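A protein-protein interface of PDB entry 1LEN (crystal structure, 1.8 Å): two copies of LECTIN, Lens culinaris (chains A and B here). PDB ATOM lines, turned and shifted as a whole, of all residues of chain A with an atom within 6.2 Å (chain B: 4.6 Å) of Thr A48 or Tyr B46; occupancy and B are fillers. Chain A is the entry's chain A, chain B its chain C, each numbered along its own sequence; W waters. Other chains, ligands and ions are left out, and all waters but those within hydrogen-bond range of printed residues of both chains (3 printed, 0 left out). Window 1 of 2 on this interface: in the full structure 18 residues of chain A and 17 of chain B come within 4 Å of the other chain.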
ATOM      1  N   THR A   3      23.693  16.336  18.098  1.00  0.00           N
ATOM      2  CA  THR A   3      22.751  17.477  17.934  1.00  0.00           C
ATOM      3  C   THR A   3      21.681  17.336  19.027  1.00  0.00           C
ATOM      4  O   THR A   3      21.473  16.227  19.500  1.00  0.00           O
ATOM      5  CB  THR A   3      22.099  17.440  16.583  1.00  0.00           C
ATOM      6  OG1 THR A   3      21.175  16.363  16.542  1.00  0.00           O
ATOM      7  CG2 THR A   3      23.113  17.273  15.504  1.00  0.00           C
ATOM      8  N   THR A   4      21.088  18.406  19.446  1.00  0.00           N
ATOM      9  CA  THR A   4      20.058  18.369  20.500  1.00  0.00           C
ATOM     10  C   THR A   4      18.994  19.396  20.103  1.00  0.00           C
ATOM     11  O   THR A   4      19.391  20.386  19.547  1.00  0.00           O
ATOM     12  CB  THR A   4      20.615  18.706  21.857  1.00  0.00           C
ATOM     13  OG1 THR A   4      21.388  17.642  22.389  1.00  0.00           O
ATOM     14  CG2 THR A   4      19.480  18.975  22.817  1.00  0.00           C
ATOM     15  N   ASN A  17      11.350  17.729  32.730  1.00  0.00           N
ATOM     16  CA  ASN A  17      12.625  17.926  32.049  1.00  0.00           C
ATOM     17  C   ASN A  17      13.233  19.271  32.388  1.00  0.00           C
ATOM     18  O   ASN A  17      14.178  19.650  31.723  1.00  0.00           O
ATOM     19  CB  ASN A  17      12.521  17.715  30.564  1.00  0.00           C
ATOM     20  CG  ASN A  17      11.409  18.490  29.913  1.00  0.00           C
ATOM     21  OD1 ASN A  17      10.643  19.267  30.613  1.00  0.00           O
ATOM     22  ND2 ASN A  17      11.173  18.403  28.619  1.00  0.00           N
ATOM     23  N   ILE A  19      14.719  21.963  35.656  1.00  0.00           N
ATOM     24  CA  ILE A  19      15.175  22.010  37.057  1.00  0.00           C
ATOM     25  C   ILE A  19      14.781  23.410  37.588  1.00  0.00           C
ATOM     26  O   ILE A  19      15.022  24.414  36.886  1.00  0.00           O
ATOM     27  CB  ILE A  19      16.650  21.779  37.194  1.00  0.00           C
ATOM     28  CG1 ILE A  19      17.056  20.391  36.721  1.00  0.00           C
ATOM     29  CG2 ILE A  19      17.168  22.024  38.604  1.00  0.00           C
ATOM     30  CD1 ILE A  19      18.492  20.299  36.317  1.00  0.00           C
ATOM     31  N   TYR A  46      17.105  23.812  31.756  1.00  0.00           N
ATOM     32  CA  TYR A  46      16.711  22.583  30.980  1.00  0.00           C
ATOM     33  C   TYR A  46      17.509  21.442  31.635  1.00  0.00           C
ATOM     34  O   TYR A  46      18.711  21.605  31.970  1.00  0.00           O
ATOM     35  CB  TYR A  46      17.104  22.726  29.539  1.00  0.00           C
ATOM     36  CG  TYR A  46      16.612  21.551  28.694  1.00  0.00           C
ATOM     37  CD1 TYR A  46      15.245  21.388  28.515  1.00  0.00           C
ATOM     38  CD2 TYR A  46      17.492  20.657  28.088  1.00  0.00           C
ATOM     39  CE1 TYR A  46      14.759  20.343  27.734  1.00  0.00           C
ATOM     40  CE2 TYR A  46      16.987  19.604  27.318  1.00  0.00           C
ATOM     41  CZ  TYR A  46      15.635  19.443  27.125  1.00  0.00           C
ATOM     42  OH  TYR A  46      15.099  18.418  26.359  1.00  0.00           O
ATOM     43  N   SER A  47      17.004  20.286  31.990  1.00  0.00           N
ATOM     44  CA  SER A  47      17.815  19.354  32.736  1.00  0.00           C
ATOM     45  C   SER A  47      18.927  18.674  32.013  1.00  0.00           C
ATOM     46  O   SER A  47      19.859  18.260  32.745  1.00  0.00           O
ATOM     47  CB  SER A  47      16.987  18.400  33.566  1.00  0.00           C
ATOM     48  OG  SER A  47      16.429  17.393  32.727  1.00  0.00           O
ATOM     49  N   THR A  48      18.955  18.480  30.744  1.00  0.00           N
ATOM     50  CA  THR A  48      20.003  17.742  30.021  1.00  0.00           C
ATOM     51  C   THR A  48      21.260  18.557  29.841  1.00  0.00           C
ATOM     52  O   THR A  48      21.216  19.682  29.352  1.00  0.00           O
ATOM     53  CB  THR A  48      19.435  17.415  28.624  1.00  0.00           C
ATOM     54  OG1 THR A  48      18.102  16.946  28.784  1.00  0.00           O
ATOM     55  CG2 THR A  48      20.273  16.377  27.970  1.00  0.00           C
ATOM     56  N   PRO A  49      22.412  17.990  30.155  1.00  0.00           N
ATOM     57  CA  PRO A  49      23.634  18.789  29.895  1.00  0.00           C
ATOM     58  C   PRO A  49      23.823  18.893  28.394  1.00  0.00           C
ATOM     59  O   PRO A  49      23.538  17.930  27.717  1.00  0.00           O
ATOM     60  CB  PRO A  49      24.673  17.877  30.493  1.00  0.00           C
ATOM     61  CG  PRO A  49      23.976  17.209  31.675  1.00  0.00           C
ATOM     62  CD  PRO A  49      22.575  16.927  31.111  1.00  0.00           C
ATOM     63  N   ILE A  50      24.239  20.046  27.955  1.00  0.00           N
ATOM     64  CA  ILE A  50      24.461  20.225  26.508  1.00  0.00           C
ATOM     65  C   ILE A  50      25.990  20.206  26.248  1.00  0.00           C
ATOM     66  O   ILE A  50      26.734  20.771  27.040  1.00  0.00           O
ATOM     67  CB  ILE A  50      23.935  21.573  26.047  1.00  0.00           C
ATOM     68  CG1 ILE A  50      22.518  21.823  26.504  1.00  0.00           C
ATOM     69  CG2 ILE A  50      24.126  21.764  24.557  1.00  0.00           C
ATOM     70  CD1 ILE A  50      21.461  20.933  25.944  1.00  0.00           C
ATOM     71  N   PHE B   6      17.495  14.306  19.249  1.00  0.00           N
ATOM     72  CA  PHE B   6      18.910  14.164  19.554  1.00  0.00           C
ATOM     73  C   PHE B   6      19.538  13.175  18.598  1.00  0.00           C
ATOM     74  O   PHE B   6      18.833  12.352  18.071  1.00  0.00           O
ATOM     75  CB  PHE B   6      19.209  13.867  20.978  1.00  0.00           C
ATOM     76  CG  PHE B   6      18.994  12.425  21.375  1.00  0.00           C
ATOM     77  CD1 PHE B   6      19.847  11.458  20.894  1.00  0.00           C
ATOM     78  CD2 PHE B   6      17.928  12.121  22.219  1.00  0.00           C
ATOM     79  CE1 PHE B   6      19.599  10.152  21.310  1.00  0.00           C
ATOM     80  CE2 PHE B   6      17.676  10.791  22.604  1.00  0.00           C
ATOM     81  CZ  PHE B   6      18.550   9.827  22.139  1.00  0.00           C
ATOM     82  N   ASN B  17      25.205  13.450  28.876  1.00  0.00           N
ATOM     83  CA  ASN B  17      23.779  13.317  28.644  1.00  0.00           C
ATOM     84  C   ASN B  17      23.321  11.880  28.693  1.00  0.00           C
ATOM     85  O   ASN B  17      22.216  11.517  28.302  1.00  0.00           O
ATOM     86  CB  ASN B  17      23.319  14.034  27.416  1.00  0.00           C
ATOM     87  CG  ASN B  17      24.123  13.596  26.206  1.00  0.00           C
ATOM     88  OD1 ASN B  17      25.015  12.687  26.413  1.00  0.00           O
ATOM     89  ND2 ASN B  17      23.950  14.116  25.032  1.00  0.00           N
ATOM     90  N   LEU B  18      24.089  10.933  29.217  1.00  0.00           N
ATOM     91  CA  LEU B  18      23.640   9.523  29.334  1.00  0.00           C
ATOM     92  C   LEU B  18      23.846   9.075  30.789  1.00  0.00           C
ATOM     93  O   LEU B  18      24.705   9.528  31.518  1.00  0.00           O
ATOM     94  CB  LEU B  18      24.509   8.628  28.443  1.00  0.00           C
ATOM     95  CG  LEU B  18      24.017   8.036  27.191  1.00  0.00           C
ATOM     96  CD1 LEU B  18      23.278   8.877  26.190  1.00  0.00           C
ATOM     97  CD2 LEU B  18      25.083   7.227  26.464  1.00  0.00           C
ATOM     98  N   ALA B  44      22.302   1.735  29.413  1.00  0.00           N
ATOM     99  CA  ALA B  44      22.612   3.150  29.171  1.00  0.00           C
ATOM    100  C   ALA B  44      21.316   3.906  28.926  1.00  0.00           C
ATOM    101  O   ALA B  44      20.603   3.476  28.001  1.00  0.00           O
ATOM    102  CB  ALA B  44      23.552   3.317  28.012  1.00  0.00           C
ATOM    103  N   LEU B  45      21.009   4.928  29.704  1.00  0.00           N
ATOM    104  CA  LEU B  45      19.765   5.645  29.465  1.00  0.00           C
ATOM    105  C   LEU B  45      19.996   7.068  28.982  1.00  0.00           C
ATOM    106  O   LEU B  45      20.905   7.741  29.356  1.00  0.00           O
ATOM    107  CB  LEU B  45      18.843   5.653  30.658  1.00  0.00           C
ATOM    108  CG  LEU B  45      18.887   4.740  31.788  1.00  0.00           C
ATOM    109  CD1 LEU B  45      17.863   5.009  32.874  1.00  0.00           C
ATOM    110  CD2 LEU B  45      19.132   3.291  31.649  1.00  0.00           C
ATOM    111  N   TYR B  46      19.141   7.565  28.120  1.00  0.00           N
ATOM    112  CA  TYR B  46      19.322   8.998  27.745  1.00  0.00           C
ATOM    113  C   TYR B  46      18.949   9.805  28.991  1.00  0.00           C
ATOM    114  O   TYR B  46      17.979   9.419  29.644  1.00  0.00           O
ATOM    115  CB  TYR B  46      18.423   9.359  26.612  1.00  0.00           C
ATOM    116  CG  TYR B  46      18.612  10.783  26.120  1.00  0.00           C
ATOM    117  CD1 TYR B  46      19.790  11.261  25.594  1.00  0.00           C
ATOM    118  CD2 TYR B  46      17.522  11.656  26.149  1.00  0.00           C
ATOM    119  CE1 TYR B  46      19.890  12.574  25.102  1.00  0.00           C
ATOM    120  CE2 TYR B  46      17.618  12.924  25.660  1.00  0.00           C
ATOM    121  CZ  TYR B  46      18.806  13.418  25.143  1.00  0.00           C
ATOM    122  OH  TYR B  46      18.831  14.699  24.676  1.00  0.00           O
ATOM    123  N   SER B  47      19.647  10.765  29.454  1.00  0.00           N
ATOM    124  CA  SER B  47      19.227  11.359  30.704  1.00  0.00           C
ATOM    125  C   SER B  47      18.002  12.215  30.637  1.00  0.00           C
ATOM    126  O   SER B  47      17.382  12.229  31.727  1.00  0.00           O
ATOM    127  CB  SER B  47      20.365  12.046  31.426  1.00  0.00           C
ATOM    128  OG  SER B  47      20.711  13.215  30.751  1.00  0.00           O
ATOM    129  N   THR B  48      17.527  12.903  29.644  1.00  0.00           N
ATOM    130  CA  THR B  48      16.318  13.734  29.708  1.00  0.00           C
ATOM    131  C   THR B  48      15.055  12.902  29.912  1.00  0.00           C
ATOM    132  O   THR B  48      14.793  11.949  29.172  1.00  0.00           O
ATOM    133  CB  THR B  48      16.150  14.440  28.353  1.00  0.00           C
ATOM    134  OG1 THR B  48      17.368  14.728  27.770  1.00  0.00           O
ATOM    135  CG2 THR B  48      15.226  15.584  28.433  1.00  0.00           C
HETATM  136  O   HOH W   1      17.275  16.651  25.574  1.00  0.00           O
HETATM  137  O   HOH W   2      22.699  16.871  25.446  1.00  0.00           O
HETATM  138  O   HOH W   3      21.198  15.245  23.762  1.00  0.00           O
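Of the printed residues of chain B, Thr A3 touches Phe B6 (3.3 Å). Thr A48 touches just these residues of chain B: Asn B17 (3.9 Å), Tyr B46 (3.97 Å) and Thr B48 (2.5 Å). Of the printed residues of chain A, Phe B6 touches Thr A3 (3.3 Å). Of chain A, only Thr A48 comes within 4 Å of Tyr B46. The nearest printed residue of chain A that does not touch Asn B17 is Thr A4 (5.1 Å).
OG1 of Thr A48 sits at hydrogen-bond distance from OG1 of Thr B48 (2.5 Å).
Water W3 lies within hydrogen-bond range of the side-chain hydroxyl (OH) of Tyr B46 (2.6 Å), the side-chain hydroxyl (OG1) of Thr A4 (2.8 Å) and the side-chain amide nitrogen (ND2) of Asn B17 (3.2 Å). Water W2 lies within hydrogen-bond range of the backbone carbonyl oxygen of Pro A49 (2.6 Å), the side-chain amide nitrogen of Asn B17 (3.1 Å) and the side-chain hydroxyl of Thr A4 (3.4 Å). Water W1 lies within hydrogen-bond range of the side-chain hydroxyl (OH) of Tyr B46 (2.7 Å), the side-chain hydroxyl (OH) of Tyr A46 (2.9 Å), the side-chain hydroxyl (OG1) of Thr B48 (2.9 Å) and the side-chain hydroxyl (OG1) of Thr A48 (3.3 Å).
Tyr A46 touches Thr B48, and with the chains exchanged Thr A48 touches Tyr B46. Thr A48 touches Asn B17, but with the chains exchanged Asn A17 does not touch Thr B48 (4.05 Å). Thr B48 touches its own counterpart, Thr A48. Of the 6 pairs that touch across the chains among the printed residues, 3 have their exchanged pair printed and touching as well.
Of the 9 printed residues of chain A, 4 touch a printed residue of chain B. Printed residues of chain A that touch a printed residue of chain B: Thr A3, Tyr A46, Thr A48 and Pro A49. Printed residues of chain B that touch a printed residue of chain A: Phe B6, Asn B17, Tyr B46 and Thr B48. Among the printed residues, no Asp or Glu carboxylate lies within 4 Å of a Lys or Arg side-chain nitrogen of the other chain.
The side-chain hydroxyl (OH) of Tyr B46 sits close to the side-chain hydroxyl (OG1) of Thr B48, 3.4 Å away. The backbone carbonyl oxygen (O) of Asn B17 sits at hydrogen-bond distance from the backbone NH (N) of Ser B47, 2.9 Å away.
Among the printed residues, merely in contact across the chains: Thr A3 with Phe B6 (3.3 Å), Tyr A46 with Thr B48 (3.5 Å), Thr A48 with Asn B17 (3.9 Å), Pro A49 with Asn B17 (3.9 Å) and Thr A48 with Tyr B46 (3.97 Å).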
